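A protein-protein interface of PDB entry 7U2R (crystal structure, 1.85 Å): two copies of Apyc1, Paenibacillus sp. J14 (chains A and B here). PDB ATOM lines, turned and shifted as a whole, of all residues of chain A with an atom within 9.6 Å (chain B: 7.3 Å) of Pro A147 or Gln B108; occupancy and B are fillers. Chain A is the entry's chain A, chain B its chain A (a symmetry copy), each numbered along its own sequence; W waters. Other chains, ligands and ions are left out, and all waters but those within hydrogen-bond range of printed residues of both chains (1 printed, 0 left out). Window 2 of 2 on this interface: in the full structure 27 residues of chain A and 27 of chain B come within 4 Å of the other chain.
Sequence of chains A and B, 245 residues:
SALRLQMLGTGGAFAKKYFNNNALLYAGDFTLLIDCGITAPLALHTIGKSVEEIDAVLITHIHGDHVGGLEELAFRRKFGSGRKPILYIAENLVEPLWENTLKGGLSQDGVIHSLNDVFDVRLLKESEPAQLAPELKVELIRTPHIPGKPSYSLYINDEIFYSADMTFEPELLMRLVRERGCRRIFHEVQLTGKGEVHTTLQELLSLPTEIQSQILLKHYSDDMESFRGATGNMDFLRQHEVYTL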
ATOM      1  N   ILE A  62     -13.865  -2.572 -24.357  1.00  0.00           N
ATOM      2  CA  ILE A  62     -12.490  -2.819 -24.787  1.00  0.00           C
ATOM      3  C   ILE A  62     -11.713  -1.501 -24.772  1.00  0.00           C
ATOM      4  O   ILE A  62     -11.842  -0.671 -25.673  1.00  0.00           O
ATOM      5  CB  ILE A  62     -12.440  -3.477 -26.165  1.00  0.00           C
ATOM      6  CG1 ILE A  62     -13.176  -4.814 -26.096  1.00  0.00           C
ATOM      7  CG2 ILE A  62     -10.993  -3.695 -26.547  1.00  0.00           C
ATOM      8  CD1 ILE A  62     -13.275  -5.464 -27.395  1.00  0.00           C
ATOM      9  N   HIS A  63     -10.873  -1.338 -23.750  1.00  0.00           N
ATOM     10  CA  HIS A  63      -9.950  -0.226 -23.592  1.00  0.00           C
ATOM     11  C   HIS A  63      -8.861  -0.741 -22.673  1.00  0.00           C
ATOM     12  O   HIS A  63      -9.129  -1.582 -21.811  1.00  0.00           O
ATOM     13  CB  HIS A  63     -10.583   0.981 -22.909  1.00  0.00           C
ATOM     14  CG  HIS A  63     -11.053   2.046 -23.829  1.00  0.00           C
ATOM     15  ND1 HIS A  63     -12.007   2.947 -23.432  1.00  0.00           N
ATOM     16  CD2 HIS A  63     -10.694   2.399 -25.086  1.00  0.00           C
ATOM     17  CE1 HIS A  63     -12.271   3.775 -24.434  1.00  0.00           C
ATOM     18  NE2 HIS A  63     -11.456   3.489 -25.434  1.00  0.00           N
ATOM     19  N   ARG A 142     -26.773  -2.062 -22.002  1.00  0.00           N
ATOM     20  CA  ARG A 142     -25.994  -1.422 -23.061  1.00  0.00           C
ATOM     21  C   ARG A 142     -26.035   0.097 -22.873  1.00  0.00           C
ATOM     22  O   ARG A 142     -27.122   0.666 -22.787  1.00  0.00           O
ATOM     23  CB  ARG A 142     -26.552  -1.826 -24.422  1.00  0.00           C
ATOM     24  CG  ARG A 142     -25.915  -1.134 -25.591  1.00  0.00           C
ATOM     25  CD  ARG A 142     -24.611  -1.752 -25.923  1.00  0.00           C
ATOM     26  NE  ARG A 142     -24.038  -1.164 -27.122  1.00  0.00           N
ATOM     27  CZ  ARG A 142     -24.119  -1.698 -28.332  1.00  0.00           C
ATOM     28  NH1 ARG A 142     -24.776  -2.827 -28.547  1.00  0.00           N
ATOM     29  NH2 ARG A 142     -23.524  -1.082 -29.352  1.00  0.00           N
ATOM     30  N   THR A 143     -24.873   0.753 -22.777  1.00  0.00           N
ATOM     31  CA  THR A 143     -24.794   2.197 -22.572  1.00  0.00           C
ATOM     32  C   THR A 143     -23.743   2.817 -23.491  1.00  0.00           C
ATOM     33  O   THR A 143     -22.863   2.112 -23.992  1.00  0.00           O
ATOM     34  CB  THR A 143     -24.471   2.539 -21.108  1.00  0.00           C
ATOM     35  OG1 THR A 143     -23.301   1.804 -20.694  1.00  0.00           O
ATOM     36  CG2 THR A 143     -25.663   2.171 -20.218  1.00  0.00           C
ATOM     37  N   PRO A 144     -23.830   4.123 -23.765  1.00  0.00           N
ATOM     38  CA  PRO A 144     -22.869   4.729 -24.704  1.00  0.00           C
ATOM     39  C   PRO A 144     -21.577   5.187 -24.038  1.00  0.00           C
ATOM     40  O   PRO A 144     -21.571   5.682 -22.913  1.00  0.00           O
ATOM     41  CB  PRO A 144     -23.656   5.931 -25.260  1.00  0.00           C
ATOM     42  CG  PRO A 144     -24.498   6.362 -24.126  1.00  0.00           C
ATOM     43  CD  PRO A 144     -24.859   5.098 -23.349  1.00  0.00           C
ATOM     44  N   HIS A 145     -20.470   5.032 -24.777  1.00  0.00           N
ATOM     45  CA  HIS A 145     -19.131   5.450 -24.381  1.00  0.00           C
ATOM     46  C   HIS A 145     -18.384   5.855 -25.654  1.00  0.00           C
ATOM     47  O   HIS A 145     -18.308   7.050 -25.969  1.00  0.00           O
ATOM     48  CB  HIS A 145     -18.467   4.316 -23.575  1.00  0.00           C
ATOM     49  CG  HIS A 145     -17.026   4.532 -23.232  1.00  0.00           C
ATOM     50  ND1 HIS A 145     -16.510   5.759 -22.850  1.00  0.00           N
ATOM     51  CD2 HIS A 145     -15.995   3.653 -23.149  1.00  0.00           C
ATOM     52  CE1 HIS A 145     -15.227   5.630 -22.576  1.00  0.00           C
ATOM     53  NE2 HIS A 145     -14.884   4.377 -22.784  1.00  0.00           N
ATOM     54  N   ILE A 146     -17.861   4.915 -26.426  1.00  0.00           N
ATOM     55  CA  ILE A 146     -17.220   5.221 -27.704  1.00  0.00           C
ATOM     56  C   ILE A 146     -18.232   4.954 -28.821  1.00  0.00           C
ATOM     57  O   ILE A 146     -18.790   3.849 -28.873  1.00  0.00           O
ATOM     58  CB  ILE A 146     -15.940   4.400 -27.928  1.00  0.00           C
ATOM     59  CG1 ILE A 146     -14.963   4.561 -26.752  1.00  0.00           C
ATOM     60  CG2 ILE A 146     -15.277   4.888 -29.222  1.00  0.00           C
ATOM     61  CD1 ILE A 146     -14.496   6.022 -26.597  1.00  0.00           C
ATOM     62  N   PRO A 147     -18.510   5.924 -29.695  1.00  0.00           N
ATOM     63  CA  PRO A 147     -19.453   5.673 -30.805  1.00  0.00           C
ATOM     64  C   PRO A 147     -19.015   4.503 -31.685  1.00  0.00           C
ATOM     65  O   PRO A 147     -17.839   4.377 -32.053  1.00  0.00           O
ATOM     66  CB  PRO A 147     -19.444   6.999 -31.580  1.00  0.00           C
ATOM     67  CG  PRO A 147     -19.008   8.033 -30.591  1.00  0.00           C
ATOM     68  CD  PRO A 147     -18.078   7.334 -29.621  1.00  0.00           C
ATOM     69  N   GLY A 148     -19.978   3.633 -32.022  1.00  0.00           N
ATOM     70  CA  GLY A 148     -19.707   2.456 -32.820  1.00  0.00           C
ATOM     71  C   GLY A 148     -19.114   1.269 -32.079  1.00  0.00           C
ATOM     72  O   GLY A 148     -18.891   0.225 -32.704  1.00  0.00           O
ATOM     73  N   LYS A 149     -18.847   1.381 -30.779  1.00  0.00           N
ATOM     74  CA  LYS A 149     -18.285   0.275 -30.003  1.00  0.00           C
ATOM     75  C   LYS A 149     -19.247  -0.129 -28.892  1.00  0.00           C
ATOM     76  O   LYS A 149     -19.759   0.746 -28.175  1.00  0.00           O
ATOM     77  CB  LYS A 149     -16.923   0.667 -29.411  1.00  0.00           C
ATOM     78  CG  LYS A 149     -15.970   1.128 -30.482  1.00  0.00           C
ATOM     79  CD  LYS A 149     -14.605   1.470 -29.913  1.00  0.00           C
ATOM     80  CE  LYS A 149     -13.596   0.371 -30.115  1.00  0.00           C
ATOM     81  NZ  LYS A 149     -12.262   0.845 -29.633  1.00  0.00           N
ATOM     82  N   PRO A 150     -19.547  -1.419 -28.734  1.00  0.00           N
ATOM     83  CA  PRO A 150     -20.438  -1.832 -27.643  1.00  0.00           C
ATOM     84  C   PRO A 150     -19.724  -1.662 -26.308  1.00  0.00           C
ATOM     85  O   PRO A 150     -18.576  -2.072 -26.151  1.00  0.00           O
ATOM     86  CB  PRO A 150     -20.716  -3.315 -27.947  1.00  0.00           C
ATOM     87  CG  PRO A 150     -20.095  -3.586 -29.280  1.00  0.00           C
ATOM     88  CD  PRO A 150     -19.020  -2.579 -29.475  1.00  0.00           C
ATOM     89  N   SER A 151     -20.406  -1.038 -25.355  1.00  0.00           N
ATOM     90  CA  SER A 151     -19.911  -0.962 -23.992  1.00  0.00           C
ATOM     91  C   SER A 151     -21.110  -1.125 -23.072  1.00  0.00           C
ATOM     92  O   SER A 151     -22.247  -0.876 -23.470  1.00  0.00           O
ATOM     93  CB  SER A 151     -19.169   0.359 -23.745  1.00  0.00           C
ATOM     94  OG  SER A 151     -20.006   1.475 -23.957  1.00  0.00           O
ATOM     95  N   THR A 167     -21.190   8.015 -21.172  1.00  0.00           N
ATOM     96  CA  THR A 167     -21.586   9.413 -21.215  1.00  0.00           C
ATOM     97  C   THR A 167     -22.884   9.593 -20.425  1.00  0.00           C
ATOM     98  O   THR A 167     -23.508   8.631 -19.977  1.00  0.00           O
ATOM     99  CB  THR A 167     -21.749   9.889 -22.664  1.00  0.00           C
ATOM    100  OG1 THR A 167     -22.478   8.911 -23.412  1.00  0.00           O
ATOM    101  CG2 THR A 167     -20.400  10.083 -23.319  1.00  0.00           C
ATOM    102  N   GLY A 195     -17.201  16.568 -21.771  1.00  0.00           N
ATOM    103  CA  GLY A 195     -17.567  15.163 -21.662  1.00  0.00           C
ATOM    104  C   GLY A 195     -17.891  14.511 -22.995  1.00  0.00           C
ATOM    105  O   GLY A 195     -19.061  14.292 -23.327  1.00  0.00           O
ATOM    106  N   GLU A 196     -16.858  14.184 -23.778  1.00  0.00           N
ATOM    107  CA  GLU A 196     -17.120  13.591 -25.086  1.00  0.00           C
ATOM    108  C   GLU A 196     -17.418  12.109 -24.962  1.00  0.00           C
ATOM    109  O   GLU A 196     -18.298  11.600 -25.656  1.00  0.00           O
ATOM    110  CB  GLU A 196     -15.935  13.799 -26.028  1.00  0.00           C
ATOM    111  CG  GLU A 196     -15.435  15.235 -26.134  1.00  0.00           C
ATOM    112  CD  GLU A 196     -14.725  15.505 -27.442  1.00  0.00           C
ATOM    113  OE1 GLU A 196     -14.819  14.648 -28.349  1.00  0.00           O
ATOM    114  OE2 GLU A 196     -14.079  16.573 -27.568  1.00  0.00           O
ATOM    115  N   VAL A 197     -16.701  11.400 -24.089  1.00  0.00           N
ATOM    116  CA  VAL A 197     -16.911   9.958 -24.003  1.00  0.00           C
ATOM    117  C   VAL A 197     -17.053   9.516 -22.549  1.00  0.00           C
ATOM    118  O   VAL A 197     -17.162   8.322 -22.281  1.00  0.00           O
ATOM    119  CB  VAL A 197     -15.775   9.184 -24.703  1.00  0.00           C
ATOM    120  CG1 VAL A 197     -15.771   9.485 -26.211  1.00  0.00           C
ATOM    121  CG2 VAL A 197     -14.410   9.479 -24.025  1.00  0.00           C
ATOM    122  N   HIS A 198     -17.138  10.481 -21.627  1.00  0.00           N
ATOM    123  CA  HIS A 198     -17.336  10.276 -20.196  1.00  0.00           C
ATOM    124  C   HIS A 198     -18.389  11.252 -19.684  1.00  0.00           C
ATOM    125  O   HIS A 198     -18.819  12.176 -20.393  1.00  0.00           O
ATOM    126  CB  HIS A 198     -16.013  10.466 -19.426  1.00  0.00           C
ATOM    127  CG  HIS A 198     -15.001   9.415 -19.746  1.00  0.00           C
ATOM    128  ND1 HIS A 198     -15.189   8.095 -19.395  1.00  0.00           N
ATOM    129  CD2 HIS A 198     -13.818   9.467 -20.404  1.00  0.00           C
ATOM    130  CE1 HIS A 198     -14.169   7.379 -19.822  1.00  0.00           C
ATOM    131  NE2 HIS A 198     -13.318   8.184 -20.434  1.00  0.00           N
ATOM    132  N   PHE B  75      -2.879   7.514 -26.924  1.00  0.00           N
ATOM    133  CA  PHE B  75      -3.992   8.411 -26.583  1.00  0.00           C
ATOM    134  C   PHE B  75      -3.489   9.674 -25.915  1.00  0.00           C
ATOM    135  O   PHE B  75      -4.024  10.756 -26.140  1.00  0.00           O
ATOM    136  CB  PHE B  75      -4.981   7.750 -25.615  1.00  0.00           C
ATOM    137  CG  PHE B  75      -6.057   6.938 -26.262  1.00  0.00           C
ATOM    138  CD1 PHE B  75      -6.791   7.429 -27.345  1.00  0.00           C
ATOM    139  CD2 PHE B  75      -6.365   5.674 -25.752  1.00  0.00           C
ATOM    140  CE1 PHE B  75      -7.798   6.651 -27.909  1.00  0.00           C
ATOM    141  CE2 PHE B  75      -7.369   4.898 -26.304  1.00  0.00           C
ATOM    142  CZ  PHE B  75      -8.086   5.374 -27.374  1.00  0.00           C
ATOM    143  N   LYS B  78      -2.060  11.885 -28.535  1.00  0.00           N
ATOM    144  CA  LYS B  78      -3.148  12.424 -29.351  1.00  0.00           C
ATOM    145  C   LYS B  78      -3.869  13.568 -28.648  1.00  0.00           C
ATOM    146  O   LYS B  78      -4.215  14.570 -29.281  1.00  0.00           O
ATOM    147  CB  LYS B  78      -4.155  11.322 -29.700  1.00  0.00           C
ATOM    148  CG  LYS B  78      -5.285  11.798 -30.632  1.00  0.00           C
ATOM    149  CD  LYS B  78      -6.433  10.777 -30.697  1.00  0.00           C
ATOM    150  CE  LYS B  78      -7.617  11.310 -31.533  1.00  0.00           C
ATOM    151  NZ  LYS B  78      -7.165  11.529 -32.934  1.00  0.00           N
ATOM    152  N   PHE B  79      -4.140  13.427 -27.351  1.00  0.00           N
ATOM    153  CA  PHE B  79      -4.893  14.448 -26.628  1.00  0.00           C
ATOM    154  C   PHE B  79      -4.015  15.565 -26.092  1.00  0.00           C
ATOM    155  O   PHE B  79      -4.554  16.571 -25.608  1.00  0.00           O
ATOM    156  CB  PHE B  79      -5.655  13.828 -25.446  1.00  0.00           C
ATOM    157  CG  PHE B  79      -6.601  12.729 -25.851  1.00  0.00           C
ATOM    158  CD1 PHE B  79      -7.259  12.783 -27.079  1.00  0.00           C
ATOM    159  CD2 PHE B  79      -6.820  11.623 -25.013  1.00  0.00           C
ATOM    160  CE1 PHE B  79      -8.122  11.743 -27.469  1.00  0.00           C
ATOM    161  CE2 PHE B  79      -7.696  10.581 -25.411  1.00  0.00           C
ATOM    162  CZ  PHE B  79      -8.332  10.648 -26.623  1.00  0.00           C
ATOM    163  N   TRP B  98      -0.920  -3.963 -34.854  1.00  0.00           N
ATOM    164  CA  TRP B  98      -2.170  -3.230 -35.023  1.00  0.00           C
ATOM    165  C   TRP B  98      -3.364  -4.182 -34.961  1.00  0.00           C
ATOM    166  O   TRP B  98      -4.243  -4.031 -34.109  1.00  0.00           O
ATOM    167  CB  TRP B  98      -2.189  -2.426 -36.345  1.00  0.00           C
ATOM    168  CG  TRP B  98      -3.549  -1.814 -36.576  1.00  0.00           C
ATOM    169  CD1 TRP B  98      -4.506  -2.209 -37.474  1.00  0.00           C
ATOM    170  CD2 TRP B  98      -4.130  -0.749 -35.814  1.00  0.00           C
ATOM    171  NE1 TRP B  98      -5.635  -1.427 -37.336  1.00  0.00           N
ATOM    172  CE2 TRP B  98      -5.431  -0.535 -36.314  1.00  0.00           C
ATOM    173  CE3 TRP B  98      -3.673   0.039 -34.749  1.00  0.00           C
ATOM    174  CZ2 TRP B  98      -6.272   0.461 -35.806  1.00  0.00           C
ATOM    175  CZ3 TRP B  98      -4.512   1.017 -34.239  1.00  0.00           C
ATOM    176  CH2 TRP B  98      -5.801   1.217 -34.773  1.00  0.00           C
ATOM    177  N   LYS B 103      -5.652  -2.508 -32.100  1.00  0.00           N
ATOM    178  CA  LYS B 103      -6.854  -2.091 -32.813  1.00  0.00           C
ATOM    179  C   LYS B 103      -8.078  -2.110 -31.910  1.00  0.00           C
ATOM    180  O   LYS B 103      -8.903  -1.201 -31.967  1.00  0.00           O
ATOM    181  CB  LYS B 103      -7.077  -2.990 -34.034  1.00  0.00           C
ATOM    182  CG  LYS B 103      -8.430  -2.832 -34.664  1.00  0.00           C
ATOM    183  CD  LYS B 103      -8.512  -3.694 -35.906  1.00  0.00           C
ATOM    184  CE  LYS B 103      -9.848  -3.578 -36.569  1.00  0.00           C
ATOM    185  NZ  LYS B 103      -9.705  -4.224 -37.869  1.00  0.00           N
ATOM    186  N   GLY B 104      -8.205  -3.115 -31.047  1.00  0.00           N
ATOM    187  CA  GLY B 104      -9.442  -3.248 -30.295  1.00  0.00           C
ATOM    188  C   GLY B 104      -9.757  -2.018 -29.465  1.00  0.00           C
ATOM    189  O   GLY B 104     -10.884  -1.509 -29.478  1.00  0.00           O
ATOM    190  N   GLY B 105      -8.763  -1.512 -28.753  1.00  0.00           N
ATOM    191  CA  GLY B 105      -8.965  -0.382 -27.861  1.00  0.00           C
ATOM    192  C   GLY B 105      -8.809   0.962 -28.552  1.00  0.00           C
ATOM    193  O   GLY B 105      -9.480   1.929 -28.195  1.00  0.00           O
ATOM    194  N   LEU B 106      -7.925   1.048 -29.534  1.00  0.00           N
ATOM    195  CA  LEU B 106      -7.634   2.353 -30.118  1.00  0.00           C
ATOM    196  C   LEU B 106      -8.595   2.738 -31.240  1.00  0.00           C
ATOM    197  O   LEU B 106      -8.862   3.932 -31.430  1.00  0.00           O
ATOM    198  CB  LEU B 106      -6.203   2.389 -30.650  1.00  0.00           C
ATOM    199  CG  LEU B 106      -5.074   2.691 -29.655  1.00  0.00           C
ATOM    200  CD1 LEU B 106      -3.740   2.537 -30.325  1.00  0.00           C
ATOM    201  CD2 LEU B 106      -5.188   4.103 -29.098  1.00  0.00           C
ATOM    202  N   SER B 107      -9.126   1.772 -31.974  1.00  0.00           N
ATOM    203  CA  SER B 107      -9.834   2.099 -33.207  1.00  0.00           C
ATOM    204  C   SER B 107     -11.149   2.788 -32.898  1.00  0.00           C
ATOM    205  O   SER B 107     -11.770   2.569 -31.857  1.00  0.00           O
ATOM    206  CB  SER B 107     -10.080   0.849 -34.043  1.00  0.00           C
ATOM    207  OG  SER B 107     -10.869  -0.074 -33.324  1.00  0.00           O
ATOM    208  N   GLN B 108     -11.560   3.661 -33.810  1.00  0.00           N
ATOM    209  CA  GLN B 108     -12.752   4.459 -33.596  1.00  0.00           C
ATOM    210  C   GLN B 108     -13.107   5.079 -34.928  1.00  0.00           C
ATOM    211  O   GLN B 108     -12.245   5.690 -35.568  1.00  0.00           O
ATOM    212  CB  GLN B 108     -12.541   5.552 -32.538  1.00  0.00           C
ATOM    213  CG  GLN B 108     -13.755   6.463 -32.469  1.00  0.00           C
ATOM    214  CD  GLN B 108     -13.677   7.473 -31.333  1.00  0.00           C
ATOM    215  OE1 GLN B 108     -12.617   7.691 -30.730  1.00  0.00           O
ATOM    216  NE2 GLN B 108     -14.814   8.114 -31.048  1.00  0.00           N
ATOM    217  N   ASP B 109     -14.379   4.928 -35.312  1.00  0.00           N
ATOM    218  CA  ASP B 109     -14.830   5.092 -36.692  1.00  0.00           C
ATOM    219  C   ASP B 109     -14.246   6.324 -37.376  1.00  0.00           C
ATOM    220  O   ASP B 109     -13.582   6.216 -38.410  1.00  0.00           O
ATOM    221  CB  ASP B 109     -16.359   5.130 -36.722  1.00  0.00           C
ATOM    222  CG  ASP B 109     -16.967   3.748 -36.806  1.00  0.00           C
ATOM    223  OD1 ASP B 109     -16.252   2.827 -37.256  1.00  0.00           O
ATOM    224  OD2 ASP B 109     -18.155   3.579 -36.444  1.00  0.00           O
ATOM    225  N   GLY B 110     -14.498   7.506 -36.855  1.00  0.00           N
ATOM    226  CA  GLY B 110     -14.092   8.630 -37.685  1.00  0.00           C
ATOM    227  C   GLY B 110     -12.698   9.144 -37.372  1.00  0.00           C
ATOM    228  O   GLY B 110     -12.307  10.215 -37.847  1.00  0.00           O
ATOM    229  N   VAL B 111     -11.928   8.380 -36.595  1.00  0.00           N
ATOM    230  CA  VAL B 111     -10.893   8.974 -35.749  1.00  0.00           C
ATOM    231  C   VAL B 111      -9.548   8.246 -35.850  1.00  0.00           C
ATOM    232  O   VAL B 111      -8.508   8.872 -36.095  1.00  0.00           O
ATOM    233  CB  VAL B 111     -11.409   9.012 -34.294  1.00  0.00           C
ATOM    234  CG1 VAL B 111     -10.320   9.475 -33.304  1.00  0.00           C
ATOM    235  CG2 VAL B 111     -12.700   9.862 -34.198  1.00  0.00           C
ATOM    236  N   ILE B 112      -9.547   6.930 -35.644  1.00  0.00           N
ATOM    237  CA  ILE B 112      -8.320   6.138 -35.697  1.00  0.00           C
ATOM    238  C   ILE B 112      -8.643   4.862 -36.457  1.00  0.00           C
ATOM    239  O   ILE B 112      -9.475   4.068 -36.007  1.00  0.00           O
ATOM    240  CB  ILE B 112      -7.764   5.802 -34.296  1.00  0.00           C
ATOM    241  CG1 ILE B 112      -7.358   7.081 -33.565  1.00  0.00           C
ATOM    242  CG2 ILE B 112      -6.570   4.867 -34.420  1.00  0.00           C
ATOM    243  CD1 ILE B 112      -7.034   6.882 -32.036  1.00  0.00           C
ATOM    244  N   HIS B 113      -7.985   4.661 -37.602  1.00  0.00           N
ATOM    245  CA  HIS B 113      -8.202   3.493 -38.446  1.00  0.00           C
ATOM    246  C   HIS B 113      -6.995   2.585 -38.555  1.00  0.00           C
ATOM    247  O   HIS B 113      -7.168   1.405 -38.862  1.00  0.00           O
ATOM    248  CB  HIS B 113      -8.588   3.903 -39.873  1.00  0.00           C
ATOM    249  CG  HIS B 113      -9.937   4.526 -39.989  1.00  0.00           C
ATOM    250  ND1 HIS B 113     -10.453   4.950 -41.197  1.00  0.00           N
ATOM    251  CD2 HIS B 113     -10.876   4.808 -39.058  1.00  0.00           C
ATOM    252  CE1 HIS B 113     -11.652   5.467 -41.004  1.00  0.00           C
ATOM    253  NE2 HIS B 113     -11.937   5.386 -39.717  1.00  0.00           N
ATOM    254  N   ASP B 117      -2.432   6.409 -37.683  1.00  0.00           N
ATOM    255  CA  ASP B 117      -3.191   7.508 -37.115  1.00  0.00           C
ATOM    256  C   ASP B 117      -2.696   7.904 -35.729  1.00  0.00           C
ATOM    257  O   ASP B 117      -3.103   8.954 -35.234  1.00  0.00           O
ATOM    258  CB  ASP B 117      -4.678   7.157 -37.042  1.00  0.00           C
ATOM    259  CG  ASP B 117      -5.338   7.078 -38.418  1.00  0.00           C
ATOM    260  OD1 ASP B 117      -5.078   7.956 -39.270  1.00  0.00           O
ATOM    261  OD2 ASP B 117      -6.124   6.131 -38.639  1.00  0.00           O
HETATM  262  O   HOH W   1     -11.325   4.005 -28.434  1.00  0.00           O
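Water W1 lies within hydrogen-bond range of O of Gly B105 (2.8 Å) and NE2 of His A63 (3.0 Å).
Gly B104 touches Ile A62 (C to CG2, 3.6 Å). Ile A62 touches Gly B105 (O to CA, 3.6 Å). CD2 of His A63 touches O of Gly B105, 3.4 Å away. CG2 of Ile A146 touches CD of Gln B108, 3.7 Å away. Pro A147 touches Gln B108.
No position is printed for both chains. Of the 8 pairs that touch across the chains among the printed residues, none has its exchanged pair printed and touching as well.
O of Lys B103 lies within hydrogen-bond range of OG of Ser B107.
Hydrophobic or aromatic side chains of chain A that line the printed part of chain B: Ile A62, His A63, Ile A146 and Pro A147. Of the 16 printed residues of chain B, 4 touch a printed residue of chain A. Among the printed residues, 8 pairs touch across the chains. Among the printed residues, no Asp or Glu carboxylate lies within 4 Å of a Lys or Arg side-chain nitrogen of the other chain.
The backbone carbonyl oxygen (O) of Gly B104 is in hydrogen-bond range of the side-chain amino group (NZ) of Lys A149, at 2.7 Å. The side-chain amino group (NZ) of Lys A149 is in hydrogen-bond range of the backbone carbonyl oxygen (O) of Gly B105, at 3.3 Å. The backbone carbonyl oxygen of Ser B107 sits at hydrogen-bond distance from the side-chain amino group of Lys A149.
Printed residues of chain B within 4 Å of Ile A62: Gly B104 and Gly B105. Of the printed residues of chain B, His A63 touches Gly B105. Printed residues of chain B within 4 Å of Ile A146: Gln B108 (3.7 Å). Pro A147 touches just one residue of chain B: Gln B108. Of the printed residues of chain B, Lys A149 touches Gly B104 (2.7 Å), Gly B105 (3.3 Å) and Ser B107 (2.9 Å). Of the printed residues of chain A, Gly B105 touches Ile A62, His A63 and Lys A149. Leu B106 touches none of the printed residues of chain A. Gln B108 touches two residues of chain A. No residue of chain A comes within 4 Å of Asp B109. No residue of chain A comes within 4 Å of Gly B110. His B113 touches none of the printed residues of chain A. The nearest residue of chain B that does not touch Pro A147 is Asp B109 (4.5 Å). The nearest residue of chain A that does not touch Gln B108 is Lys A149 (5.1 Å).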
